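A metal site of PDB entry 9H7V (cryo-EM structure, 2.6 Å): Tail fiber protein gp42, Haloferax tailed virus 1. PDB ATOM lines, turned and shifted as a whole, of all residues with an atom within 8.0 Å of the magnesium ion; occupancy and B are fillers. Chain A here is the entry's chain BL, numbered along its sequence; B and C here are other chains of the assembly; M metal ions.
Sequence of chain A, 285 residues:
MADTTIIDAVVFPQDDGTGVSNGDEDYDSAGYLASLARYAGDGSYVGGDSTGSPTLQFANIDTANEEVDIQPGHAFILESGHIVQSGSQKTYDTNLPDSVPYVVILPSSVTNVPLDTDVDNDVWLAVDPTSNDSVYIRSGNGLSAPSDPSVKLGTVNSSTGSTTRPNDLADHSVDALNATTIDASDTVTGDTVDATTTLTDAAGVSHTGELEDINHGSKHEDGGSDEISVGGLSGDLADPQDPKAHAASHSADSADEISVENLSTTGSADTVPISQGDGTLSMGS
The side-chain amide nitrogen of Gln 14 of chain A is in hydrogen-bond range of the backbone carbonyl oxygen of Ser 131, at 3.3 Å. ND2 of Asn 132 is in hydrogen-bond range of O of Asp 24 (2.7 Å). The backbone carbonyl oxygen of Asp 26 is in hydrogen-bond range of the backbone NH of Leu 14 of chain C (3.0 Å). ND2 of Asn 132 sits at hydrogen-bond distance from O of Gly 87 of chain B (3.3 Å). The backbone NH (N) of Gly 87 of chain B lies within hydrogen-bond range of the side-chain carboxylate (OD2) of Asp 133 (2.8 Å).
Of the 27 residues printed, 5 come within 4 Å of the magnesium ion. The nearest printed residue that does not touch the magnesium ion is Phe 12 (4.3 Å).
The magnesium ion is bound by OD1 of Asp 133, OD1 of Asn 132, OD1 of Asp 26, O of Val 11 and OE1 of Gln 14 of chain A. The magnesium ion has five donor atoms within binding distance. Slightly farther from the magnesium ion lies the side-chain carboxylate (OD2) of Asp 26 (2.8 Å).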
ATOM      1  N   ALA A   9      21.663   4.669  -8.263  1.00  0.00           N
ATOM      2  CA  ALA A   9      21.211   5.668  -7.300  1.00  0.00           C
ATOM      3  C   ALA A   9      19.909   5.211  -6.636  1.00  0.00           C
ATOM      4  O   ALA A   9      19.126   4.493  -7.245  1.00  0.00           O
ATOM      5  CB  ALA A   9      21.016   6.981  -8.019  1.00  0.00           C
ATOM      6  N   VAL A  10      19.700   5.642  -5.380  1.00  0.00           N
ATOM      7  CA  VAL A  10      18.451   5.376  -4.672  1.00  0.00           C
ATOM      8  C   VAL A  10      17.886   6.676  -4.088  1.00  0.00           C
ATOM      9  O   VAL A  10      18.636   7.571  -3.700  1.00  0.00           O
ATOM     10  CB  VAL A  10      18.560   4.251  -3.615  1.00  0.00           C
ATOM     11  CG1 VAL A  10      18.814   2.882  -4.235  1.00  0.00           C
ATOM     12  CG2 VAL A  10      19.571   4.545  -2.523  1.00  0.00           C
ATOM     13  N   VAL A  11      16.545   6.745  -4.031  1.00  0.00           N
ATOM     14  CA  VAL A  11      15.780   7.901  -3.577  1.00  0.00           C
ATOM     15  C   VAL A  11      14.751   7.431  -2.559  1.00  0.00           C
ATOM     16  O   VAL A  11      14.096   6.406  -2.763  1.00  0.00           O
ATOM     17  CB  VAL A  11      15.091   8.633  -4.752  1.00  0.00           C
ATOM     18  CG1 VAL A  11      14.267   9.831  -4.305  1.00  0.00           C
ATOM     19  CG2 VAL A  11      16.078   9.068  -5.829  1.00  0.00           C
ATOM     20  N   PHE A  12      14.580   8.209  -1.472  1.00  0.00           N
ATOM     21  CA  PHE A  12      13.654   7.894  -0.395  1.00  0.00           C
ATOM     22  C   PHE A  12      13.194   9.184   0.268  1.00  0.00           C
ATOM     23  O   PHE A  12      13.948  10.153   0.302  1.00  0.00           O
ATOM     24  CB  PHE A  12      14.365   6.999   0.629  1.00  0.00           C
ATOM     25  CG  PHE A  12      13.543   6.576   1.823  1.00  0.00           C
ATOM     26  CD1 PHE A  12      13.538   7.324   2.994  1.00  0.00           C
ATOM     27  CD2 PHE A  12      12.789   5.408   1.777  1.00  0.00           C
ATOM     28  CE1 PHE A  12      12.783   6.924   4.087  1.00  0.00           C
ATOM     29  CE2 PHE A  12      12.042   5.008   2.877  1.00  0.00           C
ATOM     30  CZ  PHE A  12      12.029   5.760   4.027  1.00  0.00           C
ATOM     31  N   PRO A  13      11.954   9.260   0.836  1.00  0.00           N
ATOM     32  CA  PRO A  13      10.900   8.267   0.624  1.00  0.00           C
ATOM     33  C   PRO A  13      10.008   8.577  -0.576  1.00  0.00           C
ATOM     34  O   PRO A  13       9.840   9.745  -0.933  1.00  0.00           O
ATOM     35  CB  PRO A  13      10.109   8.356   1.947  1.00  0.00           C
ATOM     36  CG  PRO A  13      10.235   9.807   2.366  1.00  0.00           C
ATOM     37  CD  PRO A  13      11.542  10.303   1.787  1.00  0.00           C
ATOM     38  N   GLN A  14       9.452   7.525  -1.185  1.00  0.00           N
ATOM     39  CA  GLN A  14       8.583   7.668  -2.346  1.00  0.00           C
ATOM     40  C   GLN A  14       7.370   6.745  -2.233  1.00  0.00           C
ATOM     41  O   GLN A  14       7.528   5.554  -1.986  1.00  0.00           O
ATOM     42  CB  GLN A  14       9.322   7.360  -3.654  1.00  0.00           C
ATOM     43  CG  GLN A  14      10.519   8.257  -3.943  1.00  0.00           C
ATOM     44  CD  GLN A  14      11.270   7.799  -5.169  1.00  0.00           C
ATOM     45  OE1 GLN A  14      12.012   6.811  -5.131  1.00  0.00           O
ATOM     46  NE2 GLN A  14      11.080   8.502  -6.268  1.00  0.00           N
ATOM     47  N   ASP A  15       6.175   7.320  -2.439  1.00  0.00           N
ATOM     48  CA  ASP A  15       4.907   6.610  -2.475  1.00  0.00           C
ATOM     49  C   ASP A  15       3.951   7.336  -3.436  1.00  0.00           C
ATOM     50  O   ASP A  15       4.386   8.201  -4.183  1.00  0.00           O
ATOM     51  CB  ASP A  15       4.327   6.435  -1.072  1.00  0.00           C
ATOM     52  CG  ASP A  15       3.967   7.730  -0.356  1.00  0.00           C
ATOM     53  OD1 ASP A  15       3.970   8.808  -0.992  1.00  0.00           O
ATOM     54  OD2 ASP A  15       3.668   7.655   0.851  1.00  0.00           O
ATOM     55  N   THR A  18       4.062  11.220  -3.170  1.00  0.00           N
ATOM     56  CA  THR A  18       5.116  11.643  -4.085  1.00  0.00           C
ATOM     57  C   THR A  18       4.690  11.197  -5.480  1.00  0.00           C
ATOM     58  O   THR A  18       3.697  10.485  -5.624  1.00  0.00           O
ATOM     59  CB  THR A  18       6.477  11.072  -3.661  1.00  0.00           C
ATOM     60  OG1 THR A  18       6.551   9.698  -4.042  1.00  0.00           O
ATOM     61  CG2 THR A  18       6.750  11.201  -2.176  1.00  0.00           C
ATOM     62  N   VAL A  20       4.846   8.657  -7.716  1.00  0.00           N
ATOM     63  CA  VAL A  20       5.062   7.297  -8.221  1.00  0.00           C
ATOM     64  C   VAL A  20       3.729   6.548  -8.279  1.00  0.00           C
ATOM     65  O   VAL A  20       2.795   6.881  -7.554  1.00  0.00           O
ATOM     66  CB  VAL A  20       6.145   6.480  -7.464  1.00  0.00           C
ATOM     67  CG1 VAL A  20       7.547   7.048  -7.536  1.00  0.00           C
ATOM     68  CG2 VAL A  20       5.759   6.087  -6.048  1.00  0.00           C
ATOM     69  N   ASP A  24       4.958   1.167  -7.144  1.00  0.00           N
ATOM     70  CA  ASP A  24       6.353   1.603  -7.171  1.00  0.00           C
ATOM     71  C   ASP A  24       6.778   2.279  -5.866  1.00  0.00           C
ATOM     72  O   ASP A  24       7.767   3.010  -5.863  1.00  0.00           O
ATOM     73  CB  ASP A  24       6.603   2.545  -8.349  1.00  0.00           C
ATOM     74  CG  ASP A  24       6.370   1.945  -9.727  1.00  0.00           C
ATOM     75  OD1 ASP A  24       6.722   0.760  -9.926  1.00  0.00           O
ATOM     76  OD2 ASP A  24       5.851   2.667 -10.600  1.00  0.00           O
ATOM     77  N   GLU A  25       6.071   2.024  -4.757  1.00  0.00           N
ATOM     78  CA  GLU A  25       6.382   2.624  -3.465  1.00  0.00           C
ATOM     79  C   GLU A  25       7.702   2.045  -2.936  1.00  0.00           C
ATOM     80  O   GLU A  25       8.002   0.892  -3.211  1.00  0.00           O
ATOM     81  CB  GLU A  25       5.258   2.352  -2.465  1.00  0.00           C
ATOM     82  CG  GLU A  25       3.873   2.737  -2.963  1.00  0.00           C
ATOM     83  CD  GLU A  25       2.732   1.818  -2.559  1.00  0.00           C
ATOM     84  OE1 GLU A  25       2.992   0.631  -2.288  1.00  0.00           O
ATOM     85  OE2 GLU A  25       1.582   2.297  -2.523  1.00  0.00           O
ATOM     86  N   ASP A  26       8.478   2.861  -2.196  1.00  0.00           N
ATOM     87  CA  ASP A  26       9.700   2.397  -1.555  1.00  0.00           C
ATOM     88  C   ASP A  26       9.361   1.463  -0.399  1.00  0.00           C
ATOM     89  O   ASP A  26       8.250   1.515   0.132  1.00  0.00           O
ATOM     90  CB  ASP A  26      10.528   3.558  -1.000  1.00  0.00           C
ATOM     91  CG  ASP A  26      11.288   4.393  -2.014  1.00  0.00           C
ATOM     92  OD1 ASP A  26      11.813   3.813  -3.002  1.00  0.00           O
ATOM     93  OD2 ASP A  26      11.376   5.620  -1.804  1.00  0.00           O
ATOM     94  N   TYR A  27      10.319   0.621  -0.010  1.00  0.00           N
ATOM     95  CA  TYR A  27      10.235  -0.188   1.203  1.00  0.00           C
ATOM     96  C   TYR A  27      10.843   0.579   2.375  1.00  0.00           C
ATOM     97  O   TYR A  27      11.749   1.385   2.175  1.00  0.00           O
ATOM     98  CB  TYR A  27      10.909  -1.551   0.983  1.00  0.00           C
ATOM     99  CG  TYR A  27      10.009  -2.587   0.351  1.00  0.00           C
ATOM    100  CD1 TYR A  27       9.870  -2.666  -1.025  1.00  0.00           C
ATOM    101  CD2 TYR A  27       9.290  -3.475   1.141  1.00  0.00           C
ATOM    102  CE1 TYR A  27       9.038  -3.616  -1.608  1.00  0.00           C
ATOM    103  CE2 TYR A  27       8.458  -4.429   0.571  1.00  0.00           C
ATOM    104  CZ  TYR A  27       8.324  -4.494  -0.809  1.00  0.00           C
ATOM    105  OH  TYR A  27       7.508  -5.423  -1.379  1.00  0.00           O
ATOM    106  N   TYR A  32      17.453   3.651   5.091  1.00  0.00           N
ATOM    107  CA  TYR A  32      16.742   4.783   4.525  1.00  0.00           C
ATOM    108  C   TYR A  32      16.246   5.717   5.634  1.00  0.00           C
ATOM    109  O   TYR A  32      16.329   6.934   5.482  1.00  0.00           O
ATOM    110  CB  TYR A  32      15.539   4.316   3.692  1.00  0.00           C
ATOM    111  CG  TYR A  32      15.796   3.796   2.304  1.00  0.00           C
ATOM    112  CD1 TYR A  32      16.601   4.461   1.393  1.00  0.00           C
ATOM    113  CD2 TYR A  32      15.139   2.647   1.873  1.00  0.00           C
ATOM    114  CE1 TYR A  32      16.787   3.972   0.100  1.00  0.00           C
ATOM    115  CE2 TYR A  32      15.312   2.150   0.594  1.00  0.00           C
ATOM    116  CZ  TYR A  32      16.139   2.815  -0.297  1.00  0.00           C
ATOM    117  OH  TYR A  32      16.317   2.323  -1.553  1.00  0.00           O
ATOM    118  N   TYR A 102      13.759  14.683  -0.106  1.00  0.00           N
ATOM    119  CA  TYR A 102      14.201  13.352  -0.500  1.00  0.00           C
ATOM    120  C   TYR A 102      15.666  13.219  -0.105  1.00  0.00           C
ATOM    121  O   TYR A 102      16.439  14.166  -0.270  1.00  0.00           O
ATOM    122  CB  TYR A 102      14.204  13.189  -2.020  1.00  0.00           C
ATOM    123  CG  TYR A 102      12.881  13.100  -2.745  1.00  0.00           C
ATOM    124  CD1 TYR A 102      11.908  12.174  -2.406  1.00  0.00           C
ATOM    125  CD2 TYR A 102      12.652  13.915  -3.853  1.00  0.00           C
ATOM    126  CE1 TYR A 102      10.713  12.096  -3.107  1.00  0.00           C
ATOM    127  CE2 TYR A 102      11.472  13.834  -4.571  1.00  0.00           C
ATOM    128  CZ  TYR A 102      10.495  12.928  -4.196  1.00  0.00           C
ATOM    129  OH  TYR A 102       9.330  12.844  -4.887  1.00  0.00           O
ATOM    130  N   VAL A 103      16.045  12.051   0.407  1.00  0.00           N
ATOM    131  CA  VAL A 103      17.452  11.690   0.483  1.00  0.00           C
ATOM    132  C   VAL A 103      17.823  10.952  -0.805  1.00  0.00           C
ATOM    133  O   VAL A 103      17.199   9.948  -1.159  1.00  0.00           O
ATOM    134  CB  VAL A 103      17.829  10.929   1.774  1.00  0.00           C
ATOM    135  CG1 VAL A 103      17.163   9.568   1.903  1.00  0.00           C
ATOM    136  CG2 VAL A 103      19.340  10.816   1.958  1.00  0.00           C
ATOM    137  N   VAL A 127      16.170  14.467  -9.463  1.00  0.00           N
ATOM    138  CA  VAL A 127      15.272  13.337  -9.246  1.00  0.00           C
ATOM    139  C   VAL A 127      14.065  13.502 -10.157  1.00  0.00           C
ATOM    140  O   VAL A 127      13.444  14.564 -10.175  1.00  0.00           O
ATOM    141  CB  VAL A 127      14.842  13.236  -7.765  1.00  0.00           C
ATOM    142  CG1 VAL A 127      13.761  12.180  -7.537  1.00  0.00           C
ATOM    143  CG2 VAL A 127      16.025  12.980  -6.849  1.00  0.00           C
ATOM    144  N   SER A 131       8.991   7.960 -11.182  1.00  0.00           N
ATOM    145  CA  SER A 131       9.437   6.583 -11.065  1.00  0.00           C
ATOM    146  C   SER A 131      10.336   6.436  -9.834  1.00  0.00           C
ATOM    147  O   SER A 131      10.962   7.399  -9.410  1.00  0.00           O
ATOM    148  CB  SER A 131      10.161   6.149 -12.320  1.00  0.00           C
ATOM    149  OG  SER A 131      10.424   4.746 -12.287  1.00  0.00           O
ATOM    150  N   ASN A 132      10.363   5.221  -9.283  1.00  0.00           N
ATOM    151  CA  ASN A 132      11.142   4.931  -8.091  1.00  0.00           C
ATOM    152  C   ASN A 132      12.622   4.918  -8.444  1.00  0.00           C
ATOM    153  O   ASN A 132      13.035   4.192  -9.348  1.00  0.00           O
ATOM    154  CB  ASN A 132      10.679   3.642  -7.410  1.00  0.00           C
ATOM    155  CG  ASN A 132      11.123   3.521  -5.964  1.00  0.00           C
ATOM    156  OD1 ASN A 132      12.131   4.106  -5.563  1.00  0.00           O
ATOM    157  ND2 ASN A 132      10.379   2.776  -5.169  1.00  0.00           N
ATOM    158  N   ASP A 133      13.397   5.768  -7.745  1.00  0.00           N
ATOM    159  CA  ASP A 133      14.851   5.811  -7.771  1.00  0.00           C
ATOM    160  C   ASP A 133      15.413   6.229  -9.141  1.00  0.00           C
ATOM    161  O   ASP A 133      16.517   5.822  -9.492  1.00  0.00           O
ATOM    162  CB  ASP A 133      15.472   4.502  -7.249  1.00  0.00           C
ATOM    163  CG  ASP A 133      15.214   4.216  -5.774  1.00  0.00           C
ATOM    164  OD1 ASP A 133      14.637   5.091  -5.096  1.00  0.00           O
ATOM    165  OD2 ASP A 133      15.603   3.134  -5.327  1.00  0.00           O
ATOM    166  N   SER A 134      14.675   7.056  -9.888  1.00  0.00           N
ATOM    167  CA  SER A 134      15.177   7.580 -11.157  1.00  0.00           C
ATOM    168  C   SER A 134      15.913   8.895 -10.935  1.00  0.00           C
ATOM    169  O   SER A 134      15.281   9.941 -10.765  1.00  0.00           O
ATOM    170  CB  SER A 134      14.086   7.681 -12.198  1.00  0.00           C
ATOM    171  OG  SER A 134      12.925   8.310 -11.669  1.00  0.00           O
ATOM    172  N   VAL A 135      17.253   8.830 -10.933  1.00  0.00           N
ATOM    173  CA  VAL A 135      18.135   9.976 -10.717  1.00  0.00           C
ATOM    174  C   VAL A 135      18.930  10.226 -11.995  1.00  0.00           C
ATOM    175  O   VAL A 135      19.328   9.280 -12.674  1.00  0.00           O
ATOM    176  CB  VAL A 135      19.062   9.766  -9.505  1.00  0.00           C
ATOM    177  CG1 VAL A 135      19.865  11.008  -9.169  1.00  0.00           C
ATOM    178  CG2 VAL A 135      18.300   9.303  -8.275  1.00  0.00           C
ATOM    179  N   GLN B  85      17.111  -1.555   0.407  1.00  0.00           N
ATOM    180  CA  GLN B  85      16.331  -2.194  -0.644  1.00  0.00           C
ATOM    181  C   GLN B  85      16.065  -1.183  -1.760  1.00  0.00           C
ATOM    182  O   GLN B  85      15.334  -0.214  -1.546  1.00  0.00           O
ATOM    183  CB  GLN B  85      15.007  -2.716  -0.063  1.00  0.00           C
ATOM    184  CG  GLN B  85      15.156  -3.724   1.062  1.00  0.00           C
ATOM    185  CD  GLN B  85      13.950  -3.795   1.969  1.00  0.00           C
ATOM    186  OE1 GLN B  85      13.594  -2.839   2.648  1.00  0.00           O
ATOM    187  NE2 GLN B  85      13.305  -4.957   1.984  1.00  0.00           N
ATOM    188  N   SER B  86      16.661  -1.402  -2.938  1.00  0.00           N
ATOM    189  CA  SER B  86      16.534  -0.495  -4.064  1.00  0.00           C
ATOM    190  C   SER B  86      15.131  -0.577  -4.657  1.00  0.00           C
ATOM    191  O   SER B  86      14.561  -1.660  -4.779  1.00  0.00           O
ATOM    192  CB  SER B  86      17.575  -0.758  -5.121  1.00  0.00           C
ATOM    193  OG  SER B  86      17.427   0.116  -6.226  1.00  0.00           O
ATOM    194  N   GLY B  87      14.584   0.599  -5.000  1.00  0.00           N
ATOM    195  CA  GLY B  87      13.332   0.742  -5.731  1.00  0.00           C
ATOM    196  C   GLY B  87      12.179  -0.019  -5.082  1.00  0.00           C
ATOM    197  O   GLY B  87      11.905   0.150  -3.888  1.00  0.00           O
ATOM    198  N   SER B  88      11.525  -0.864  -5.883  1.00  0.00           N
ATOM    199  CA  SER B  88      10.328  -1.599  -5.496  1.00  0.00           C
ATOM    200  C   SER B  88      10.662  -3.021  -5.024  1.00  0.00           C
ATOM    201  O   SER B  88       9.764  -3.829  -4.848  1.00  0.00           O
ATOM    202  CB  SER B  88       9.335  -1.645  -6.651  1.00  0.00           C
ATOM    203  OG  SER B  88       9.287  -0.403  -7.341  1.00  0.00           O
ATOM    204  N   LEU C  14       5.868   1.596   1.942  1.00  0.00           N
ATOM    205  CA  LEU C  14       5.317   2.643   2.778  1.00  0.00           C
ATOM    206  C   LEU C  14       4.045   3.235   2.169  1.00  0.00           C
ATOM    207  O   LEU C  14       3.946   3.405   0.957  1.00  0.00           O
ATOM    208  CB  LEU C  14       6.358   3.698   3.200  1.00  0.00           C
ATOM    209  CG  LEU C  14       7.472   4.080   2.218  1.00  0.00           C
ATOM    210  CD1 LEU C  14       6.931   4.865   1.048  1.00  0.00           C
ATOM    211  CD2 LEU C  14       8.527   4.911   2.936  1.00  0.00           C
HETATM  212 MG    MG M   1      12.965   5.161  -4.044  1.00  0.00          MG
